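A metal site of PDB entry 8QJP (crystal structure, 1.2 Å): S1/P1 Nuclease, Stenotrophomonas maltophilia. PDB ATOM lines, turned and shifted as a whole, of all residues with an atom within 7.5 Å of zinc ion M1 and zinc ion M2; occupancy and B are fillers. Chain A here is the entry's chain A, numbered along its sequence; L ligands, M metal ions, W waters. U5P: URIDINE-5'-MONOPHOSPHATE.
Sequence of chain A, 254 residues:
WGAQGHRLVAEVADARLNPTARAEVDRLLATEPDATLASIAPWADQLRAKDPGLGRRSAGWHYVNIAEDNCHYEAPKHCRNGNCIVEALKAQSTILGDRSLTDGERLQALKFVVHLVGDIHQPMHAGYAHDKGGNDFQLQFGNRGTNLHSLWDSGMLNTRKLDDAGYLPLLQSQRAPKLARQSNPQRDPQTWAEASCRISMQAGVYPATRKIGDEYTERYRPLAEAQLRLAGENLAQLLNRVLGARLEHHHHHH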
ATOM      1  N   TRP A   1      -6.080 -16.840   9.109  1.00  0.00           N
ATOM      2  CA  TRP A   1      -5.795 -18.201   8.642  1.00  0.00           C
ATOM      3  C   TRP A   1      -5.085 -18.118   7.314  1.00  0.00           C
ATOM      4  O   TRP A   1      -5.198 -17.097   6.599  1.00  0.00           O
ATOM      5  CB  TRP A   1      -7.089 -19.035   8.452  1.00  0.00           C
ATOM      6  CG  TRP A   1      -7.962 -19.108   9.661  1.00  0.00           C
ATOM      7  CD1 TRP A   1      -9.038 -18.328   9.950  1.00  0.00           C
ATOM      8  CD2 TRP A   1      -7.820 -20.011  10.765  1.00  0.00           C
ATOM      9  NE1 TRP A   1      -9.613 -18.705  11.130  1.00  0.00           N
ATOM     10  CE2 TRP A   1      -8.880 -19.735  11.670  1.00  0.00           C
ATOM     11  CE3 TRP A   1      -6.932 -21.050  11.062  1.00  0.00           C
ATOM     12  CZ2 TRP A   1      -9.059 -20.437  12.846  1.00  0.00           C
ATOM     13  CZ3 TRP A   1      -7.120 -21.760  12.207  1.00  0.00           C
ATOM     14  CH2 TRP A   1      -8.148 -21.434  13.097  1.00  0.00           C
ATOM     15  N   GLY A   2      -4.441 -19.219   6.942  1.00  0.00           N
ATOM     16  CA  GLY A   2      -4.044 -19.459   5.548  1.00  0.00           C
ATOM     17  C   GLY A   2      -5.233 -19.849   4.706  1.00  0.00           C
ATOM     18  O   GLY A   2      -6.384 -19.880   5.198  1.00  0.00           O
ATOM     19  N   ALA A   3      -4.996 -20.175   3.448  1.00  0.00           N
ATOM     20  CA  ALA A   3      -6.074 -20.328   2.464  1.00  0.00           C
ATOM     21  C   ALA A   3      -6.998 -21.489   2.870  1.00  0.00           C
ATOM     22  O   ALA A   3      -8.222 -21.338   2.776  1.00  0.00           O
ATOM     23  CB  ALA A   3      -5.495 -20.501   1.074  1.00  0.00           C
ATOM     24  N   GLY A   5      -7.702 -22.792   5.849  1.00  0.00           N
ATOM     25  CA  GLY A   5      -8.602 -22.430   6.969  1.00  0.00           C
ATOM     26  C   GLY A   5      -9.741 -21.547   6.468  1.00  0.00           C
ATOM     27  O   GLY A   5     -10.889 -21.743   6.862  1.00  0.00           O
ATOM     28  N   HIS A   6      -9.445 -20.573   5.614  1.00  0.00           N
ATOM     29  CA  HIS A   6     -10.502 -19.690   5.087  1.00  0.00           C
ATOM     30  C   HIS A   6     -11.551 -20.474   4.282  1.00  0.00           C
ATOM     31  O   HIS A   6     -12.750 -20.267   4.464  1.00  0.00           O
ATOM     32  CB  HIS A   6      -9.925 -18.541   4.259  1.00  0.00           C
ATOM     33  CG  HIS A   6      -9.349 -17.505   5.161  1.00  0.00           C
ATOM     34  ND1 HIS A   6     -10.162 -16.705   5.938  1.00  0.00           N
ATOM     35  CD2 HIS A   6      -8.079 -17.168   5.464  1.00  0.00           C
ATOM     36  CE1 HIS A   6      -9.381 -15.914   6.678  1.00  0.00           C
ATOM     37  NE2 HIS A   6      -8.089 -16.199   6.437  1.00  0.00           N
ATOM     38  N   ALA A  41     -13.071 -17.336  -0.425  1.00  0.00           N
ATOM     39  CA  ALA A  41     -12.749 -17.116   1.000  1.00  0.00           C
ATOM     40  C   ALA A  41     -11.329 -16.584   1.191  1.00  0.00           C
ATOM     41  O   ALA A  41     -11.136 -15.763   2.079  1.00  0.00           O
ATOM     42  CB  ALA A  41     -13.007 -18.349   1.822  1.00  0.00           C
ATOM     43  N   PRO A  42     -10.301 -17.028   0.436  1.00  0.00           N
ATOM     44  CA  PRO A  42      -8.958 -16.493   0.583  1.00  0.00           C
ATOM     45  C   PRO A  42      -8.685 -15.166  -0.123  1.00  0.00           C
ATOM     46  O   PRO A  42      -7.613 -14.598   0.040  1.00  0.00           O
ATOM     47  CB  PRO A  42      -8.066 -17.581  -0.075  1.00  0.00           C
ATOM     48  CG  PRO A  42      -8.925 -18.819  -0.121  1.00  0.00           C
ATOM     49  CD  PRO A  42     -10.304 -18.276  -0.383  1.00  0.00           C
ATOM     50  N   ALA A  44      -9.307 -12.005   0.088  1.00  0.00           N
ATOM     51  CA  ALA A  44      -8.853 -10.763   0.723  1.00  0.00           C
ATOM     52  C   ALA A  44      -7.358 -10.828   1.018  1.00  0.00           C
ATOM     53  O   ALA A  44      -6.759  -9.773   1.179  1.00  0.00           O
ATOM     54  CB  ALA A  44      -9.660 -10.478   1.954  1.00  0.00           C
ATOM     55  N   ASP A  45      -6.777 -12.028   1.199  1.00  0.00           N
ATOM     56  CA  ASP A  45      -5.300 -12.170   1.428  1.00  0.00           C
ATOM     57  C   ASP A  45      -4.492 -12.051   0.137  1.00  0.00           C
ATOM     58  O   ASP A  45      -3.244 -11.932   0.237  1.00  0.00           O
ATOM     59  CB  ASP A  45      -4.991 -13.484   2.129  1.00  0.00           C
ATOM     60  CG  ASP A  45      -5.258 -13.530   3.615  1.00  0.00           C
ATOM     61  OD1 ASP A  45      -5.536 -12.487   4.216  1.00  0.00           O
ATOM     62  OD2 ASP A  45      -5.230 -14.644   4.210  1.00  0.00           O
ATOM     63  N   GLN A  46      -5.137 -12.100  -1.016  1.00  0.00           N
ATOM     64  CA  GLN A  46      -4.462 -12.188  -2.336  1.00  0.00           C
ATOM     65  C   GLN A  46      -4.370 -10.811  -3.010  1.00  0.00           C
ATOM     66  O   GLN A  46      -3.894 -10.767  -4.133  1.00  0.00           O
ATOM     67  CB  GLN A  46      -5.201 -13.224  -3.186  1.00  0.00           C
ATOM     68  CG  GLN A  46      -5.219 -14.620  -2.569  1.00  0.00           C
ATOM     69  CD  GLN A  46      -6.127 -15.602  -3.257  1.00  0.00           C
ATOM     70  OE1 GLN A  46      -7.160 -15.237  -3.829  1.00  0.00           O
ATOM     71  NE2 GLN A  46      -5.760 -16.882  -3.203  1.00  0.00           N
ATOM     72  N   ALA A  59      -5.340  -3.909   4.452  1.00  0.00           N
ATOM     73  CA  ALA A  59      -4.361  -4.809   5.114  1.00  0.00           C
ATOM     74  C   ALA A  59      -4.640  -4.927   6.626  1.00  0.00           C
ATOM     75  O   ALA A  59      -4.592  -6.060   7.201  1.00  0.00           O
ATOM     76  CB  ALA A  59      -2.956  -4.353   4.849  1.00  0.00           C
ATOM     77  N   TRP A  61      -7.369  -4.633   8.157  1.00  0.00           N
ATOM     78  CA  TRP A  61      -8.726  -5.142   8.452  1.00  0.00           C
ATOM     79  C   TRP A  61      -8.676  -6.599   8.909  1.00  0.00           C
ATOM     80  O   TRP A  61      -9.710  -7.089   9.324  1.00  0.00           O
ATOM     81  CB  TRP A  61      -9.626  -5.024   7.232  1.00  0.00           C
ATOM     82  CG  TRP A  61      -9.876  -3.643   6.749  1.00  0.00           C
ATOM     83  CD1 TRP A  61      -9.331  -2.462   7.194  1.00  0.00           C
ATOM     84  CD2 TRP A  61     -10.719  -3.332   5.642  1.00  0.00           C
ATOM     85  NE1 TRP A  61      -9.843  -1.424   6.457  1.00  0.00           N
ATOM     86  CE2 TRP A  61     -10.687  -1.931   5.488  1.00  0.00           C
ATOM     87  CE3 TRP A  61     -11.512  -4.095   4.773  1.00  0.00           C
ATOM     88  CZ2 TRP A  61     -11.410  -1.287   4.487  1.00  0.00           C
ATOM     89  CZ3 TRP A  61     -12.216  -3.452   3.783  1.00  0.00           C
ATOM     90  CH2 TRP A  61     -12.176  -2.064   3.658  1.00  0.00           C
ATOM     91  N   HIS A  62      -7.527  -7.258   8.771  1.00  0.00           N
ATOM     92  CA  HIS A  62      -7.467  -8.716   9.058  1.00  0.00           C
ATOM     93  C   HIS A  62      -7.277  -9.009  10.538  1.00  0.00           C
ATOM     94  O   HIS A  62      -7.327 -10.209  10.893  1.00  0.00           O
ATOM     95  CB  HIS A  62      -6.398  -9.387   8.222  1.00  0.00           C
ATOM     96  CG  HIS A  62      -6.664  -9.335   6.765  1.00  0.00           C
ATOM     97  ND1 HIS A  62      -6.737 -10.473   5.978  1.00  0.00           N
ATOM     98  CD2 HIS A  62      -6.799  -8.267   5.941  1.00  0.00           C
ATOM     99  CE1 HIS A  62      -6.999 -10.092   4.729  1.00  0.00           C
ATOM    100  NE2 HIS A  62      -7.035  -8.737   4.689  1.00  0.00           N
ATOM    101  N   TYR A  63      -7.008  -8.016  11.369  1.00  0.00           N
ATOM    102  CA  TYR A  63      -6.674  -8.316  12.777  1.00  0.00           C
ATOM    103  C   TYR A  63      -7.029  -7.160  13.700  1.00  0.00           C
ATOM    104  O   TYR A  63      -7.426  -6.089  13.253  1.00  0.00           O
ATOM    105  CB  TYR A  63      -5.214  -8.702  12.892  1.00  0.00           C
ATOM    106  CG  TYR A  63      -4.306  -7.636  12.390  1.00  0.00           C
ATOM    107  CD1 TYR A  63      -3.977  -7.548  11.050  1.00  0.00           C
ATOM    108  CD2 TYR A  63      -3.750  -6.709  13.265  1.00  0.00           C
ATOM    109  CE1 TYR A  63      -3.153  -6.523  10.611  1.00  0.00           C
ATOM    110  CE2 TYR A  63      -2.908  -5.706  12.845  1.00  0.00           C
ATOM    111  CZ  TYR A  63      -2.599  -5.607  11.505  1.00  0.00           C
ATOM    112  OH  TYR A  63      -1.760  -4.587  11.137  1.00  0.00           O
ATOM    113  N   ILE A  85     -10.166  -5.381  12.317  1.00  0.00           N
ATOM    114  CA  ILE A  85     -11.169  -6.376  11.884  1.00  0.00           C
ATOM    115  C   ILE A  85     -12.532  -6.120  12.490  1.00  0.00           C
ATOM    116  O   ILE A  85     -13.524  -6.475  11.872  1.00  0.00           O
ATOM    117  CB  ILE A  85     -10.657  -7.790  12.160  1.00  0.00           C
ATOM    118  CG1 ILE A  85     -11.523  -8.830  11.422  1.00  0.00           C
ATOM    119  CG2 ILE A  85     -10.537  -8.102  13.645  1.00  0.00           C
ATOM    120  CD1 ILE A  85     -10.819 -10.129  11.194  1.00  0.00           C
ATOM    121  N   HIS A 115     -14.149 -13.771   4.506  1.00  0.00           N
ATOM    122  CA  HIS A 115     -12.744 -13.844   4.955  1.00  0.00           C
ATOM    123  C   HIS A 115     -12.651 -13.424   6.428  1.00  0.00           C
ATOM    124  O   HIS A 115     -11.957 -14.057   7.227  1.00  0.00           O
ATOM    125  CB  HIS A 115     -11.877 -12.947   4.081  1.00  0.00           C
ATOM    126  CG  HIS A 115     -10.433 -13.111   4.357  1.00  0.00           C
ATOM    127  ND1 HIS A 115      -9.680 -14.058   3.709  1.00  0.00           N
ATOM    128  CD2 HIS A 115      -9.591 -12.498   5.222  1.00  0.00           C
ATOM    129  CE1 HIS A 115      -8.432 -13.998   4.157  1.00  0.00           C
ATOM    130  NE2 HIS A 115      -8.341 -13.039   5.106  1.00  0.00           N
ATOM    131  N   LEU A 116     -13.260 -12.259   6.715  1.00  0.00           N
ATOM    132  CA  LEU A 116     -13.066 -11.642   8.033  1.00  0.00           C
ATOM    133  C   LEU A 116     -13.753 -12.443   9.134  1.00  0.00           C
ATOM    134  O   LEU A 116     -13.228 -12.461  10.257  1.00  0.00           O
ATOM    135  CB  LEU A 116     -13.462 -10.174   8.017  1.00  0.00           C
ATOM    136  CG  LEU A 116     -12.633  -9.264   7.101  1.00  0.00           C
ATOM    137  CD1 LEU A 116     -13.145  -7.839   7.177  1.00  0.00           C
ATOM    138  CD2 LEU A 116     -11.147  -9.309   7.386  1.00  0.00           C
ATOM    139  N   GLY A 118     -13.708 -15.562   9.201  1.00  0.00           N
ATOM    140  CA  GLY A 118     -12.627 -16.523   9.475  1.00  0.00           C
ATOM    141  C   GLY A 118     -11.546 -15.883  10.354  1.00  0.00           C
ATOM    142  O   GLY A 118     -11.173 -16.444  11.380  1.00  0.00           O
ATOM    143  N   ASP A 119     -10.971 -14.765   9.906  1.00  0.00           N
ATOM    144  CA  ASP A 119      -9.809 -14.167  10.597  1.00  0.00           C
ATOM    145  C   ASP A 119     -10.156 -13.769  12.033  1.00  0.00           C
ATOM    146  O   ASP A 119      -9.297 -13.888  12.919  1.00  0.00           O
ATOM    147  CB  ASP A 119      -9.255 -12.962   9.851  1.00  0.00           C
ATOM    148  CG  ASP A 119      -8.209 -13.301   8.821  1.00  0.00           C
ATOM    149  OD1 ASP A 119      -7.767 -14.508   8.803  1.00  0.00           O
ATOM    150  OD2 ASP A 119      -7.866 -12.409   7.976  1.00  0.00           O
ATOM    151  N   ILE A 120     -11.377 -13.337  12.305  1.00  0.00           N
ATOM    152  CA  ILE A 120     -11.717 -12.844  13.655  1.00  0.00           C
ATOM    153  C   ILE A 120     -11.863 -14.007  14.638  1.00  0.00           C
ATOM    154  O   ILE A 120     -11.928 -13.760  15.831  1.00  0.00           O
ATOM    155  CB  ILE A 120     -12.971 -11.933  13.590  1.00  0.00           C
ATOM    156  CG1 ILE A 120     -13.034 -10.964  14.782  1.00  0.00           C
ATOM    157  CG2 ILE A 120     -14.252 -12.763  13.521  1.00  0.00           C
ATOM    158  CD1 ILE A 120     -14.057  -9.849  14.600  1.00  0.00           C
ATOM    159  N   GLN A 122      -9.444 -16.498  14.377  1.00  0.00           N
ATOM    160  CA  GLN A 122      -8.056 -16.974  14.493  1.00  0.00           C
ATOM    161  C   GLN A 122      -7.413 -16.296  15.691  1.00  0.00           C
ATOM    162  O   GLN A 122      -7.252 -15.075  15.675  1.00  0.00           O
ATOM    163  CB  GLN A 122      -7.354 -16.672  13.186  1.00  0.00           C
ATOM    164  CG  GLN A 122      -5.849 -16.768  13.289  1.00  0.00           C
ATOM    165  CD  GLN A 122      -5.365 -18.049  13.912  1.00  0.00           C
ATOM    166  OE1 GLN A 122      -4.714 -18.044  14.953  1.00  0.00           O
ATOM    167  NE2 GLN A 122      -5.727 -19.162  13.280  1.00  0.00           N
ATOM    168  N   HIS A 125      -4.865 -13.568  15.192  1.00  0.00           N
ATOM    169  CA  HIS A 125      -5.380 -12.326  14.566  1.00  0.00           C
ATOM    170  C   HIS A 125      -6.026 -11.402  15.610  1.00  0.00           C
ATOM    171  O   HIS A 125      -6.567 -10.352  15.213  1.00  0.00           O
ATOM    172  CB  HIS A 125      -6.320 -12.662  13.410  1.00  0.00           C
ATOM    173  CG  HIS A 125      -5.583 -13.055  12.158  1.00  0.00           C
ATOM    174  ND1 HIS A 125      -5.733 -12.397  10.950  1.00  0.00           N
ATOM    175  CD2 HIS A 125      -4.654 -14.046  11.919  1.00  0.00           C
ATOM    176  CE1 HIS A 125      -4.927 -12.919  10.037  1.00  0.00           C
ATOM    177  NE2 HIS A 125      -4.235 -13.950  10.595  1.00  0.00           N
ATOM    178  N   HIS A 149       2.422 -17.248  14.782  1.00  0.00           N
ATOM    179  CA  HIS A 149       1.316 -16.796  13.929  1.00  0.00           C
ATOM    180  C   HIS A 149       1.022 -17.835  12.833  1.00  0.00           C
ATOM    181  O   HIS A 149      -0.099 -18.284  12.693  1.00  0.00           O
ATOM    182  CB  HIS A 149       1.583 -15.407  13.356  1.00  0.00           C
ATOM    183  CG  HIS A 149       0.389 -14.853  12.663  1.00  0.00           C
ATOM    184  ND1 HIS A 149      -0.441 -13.943  13.255  1.00  0.00           N
ATOM    185  CD2 HIS A 149      -0.114 -15.100  11.427  1.00  0.00           C
ATOM    186  CE1 HIS A 149      -1.421 -13.665  12.430  1.00  0.00           C
ATOM    187  NE2 HIS A 149      -1.266 -14.346  11.279  1.00  0.00           N
ATOM    188  N   ASP A 153      -2.167 -20.136  11.892  1.00  0.00           N
ATOM    189  CA  ASP A 153      -2.850 -19.907  10.600  1.00  0.00           C
ATOM    190  C   ASP A 153      -2.913 -21.174   9.777  1.00  0.00           C
ATOM    191  O   ASP A 153      -3.918 -21.373   9.075  1.00  0.00           O
ATOM    192  CB  ASP A 153      -2.163 -18.810   9.766  1.00  0.00           C
ATOM    193  CG  ASP A 153      -2.663 -17.383   9.983  1.00  0.00           C
ATOM    194  OD1 ASP A 153      -3.568 -17.184  10.793  1.00  0.00           O
ATOM    195  OD2 ASP A 153      -2.110 -16.494   9.340  1.00  0.00           O
HETATM  196  N1  U5P L   1      -1.083  -9.522  10.172  1.00  0.00           N
HETATM  197  C2  U5P L   1      -1.727 -10.004  11.292  1.00  0.00           C
HETATM  198  N3  U5P L   1      -1.365  -9.402  12.479  1.00  0.00           N
HETATM  199  C4  U5P L   1      -0.456  -8.381  12.646  1.00  0.00           C
HETATM  200  C5  U5P L   1       0.221  -7.975  11.444  1.00  0.00           C
HETATM  201  C6  U5P L   1      -0.111  -8.548  10.260  1.00  0.00           C
HETATM  202  O2  U5P L   1      -2.620 -10.852  11.255  1.00  0.00           O
HETATM  203  O4  U5P L   1      -0.292  -7.903  13.765  1.00  0.00           O
HETATM  204  C1' U5P L   1      -1.465 -10.095   8.825  1.00  0.00           C
HETATM  205  C2' U5P L   1      -2.757  -9.508   8.289  1.00  0.00           C
HETATM  206  O2' U5P L   1      -3.455 -10.543   7.591  1.00  0.00           O
HETATM  207  C3' U5P L   1      -2.254  -8.422   7.343  1.00  0.00           C
HETATM  208  C4' U5P L   1      -1.009  -9.068   6.759  1.00  0.00           C
HETATM  209  O3' U5P L   1      -3.139  -8.093   6.285  1.00  0.00           O
HETATM  210  O4' U5P L   1      -0.464  -9.816   7.865  1.00  0.00           O
HETATM  211  C5' U5P L   1       0.022  -8.139   6.177  1.00  0.00           C
HETATM  212  O5' U5P L   1       0.392  -7.145   7.154  1.00  0.00           O
HETATM  213  P   U5P L   1       1.645  -6.236   6.885  1.00  0.00           P
HETATM  214  O1P U5P L   1       1.519  -5.073   7.832  1.00  0.00           O
HETATM  215  O2P U5P L   1       1.576  -5.766   5.431  1.00  0.00           O
HETATM  216  O3P U5P L   1       2.887  -7.109   6.982  1.00  0.00           O
HETATM  217 ZN    ZN M   1      -6.497 -15.517   7.520  1.00  0.00          ZN
HETATM  218 ZN    ZN M   2      -6.715 -12.481   6.244  1.00  0.00          ZN
HETATM  219 ZN    ZN M   3      -2.558 -14.670   9.792  1.00  0.00          ZN
HETATM  220  O   HOH W   1      -5.601 -13.959   6.833  1.00  0.00           O
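Zinc ion M1 is bound by water W1, 1.9 Å away.
Zinc ion M1 is bound by NE2 of His 6 (2.0 Å).
OD1 of Asp 119 is bound to zinc ion M1 (2.1 Å).
Zinc ion M1 is bound by N of Trp 1 (2.1 Å).
The backbone carbonyl oxygen (O) of Trp 1 binds zinc ion M1, at 2.2 Å.
Merely in contact with zinc ion M1: His 125.
Along chain A the residues within 4 Å of zinc ion M2 span positions 6 to 119.
The backbone carbonyl oxygen (O) of Ala 41 sits at hydrogen-bond distance from a ring nitrogen (ND1) of His 115, at 2.8 Å.
NE1 of Trp 1 lies within hydrogen-bond range of O of Gly 118 (2.8 Å).
The backbone carbonyl oxygen (O) of His 115 lies close to a ring nitrogen (ND1) of His 6 (3.4 Å).
The backbone NH of Trp 1 sits close to the side-chain carboxylate of Asp 153 (3.0 Å).
ND1 of His 125 sits at hydrogen-bond distance from O of His 62 (2.7 Å).
O3' of the ligand is in hydrogen-bond range of O of Ala 59, 2.7 Å away.
A ring nitrogen (ND1) of His 125 sits close to an oxygen (O2) of the ligand, at 3.5 Å.
Zinc ion M2 is bound by water W1, ND1 of His 62, NE2 of His 115, OD2 of Asp 119 and OD1 of Asp 45.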
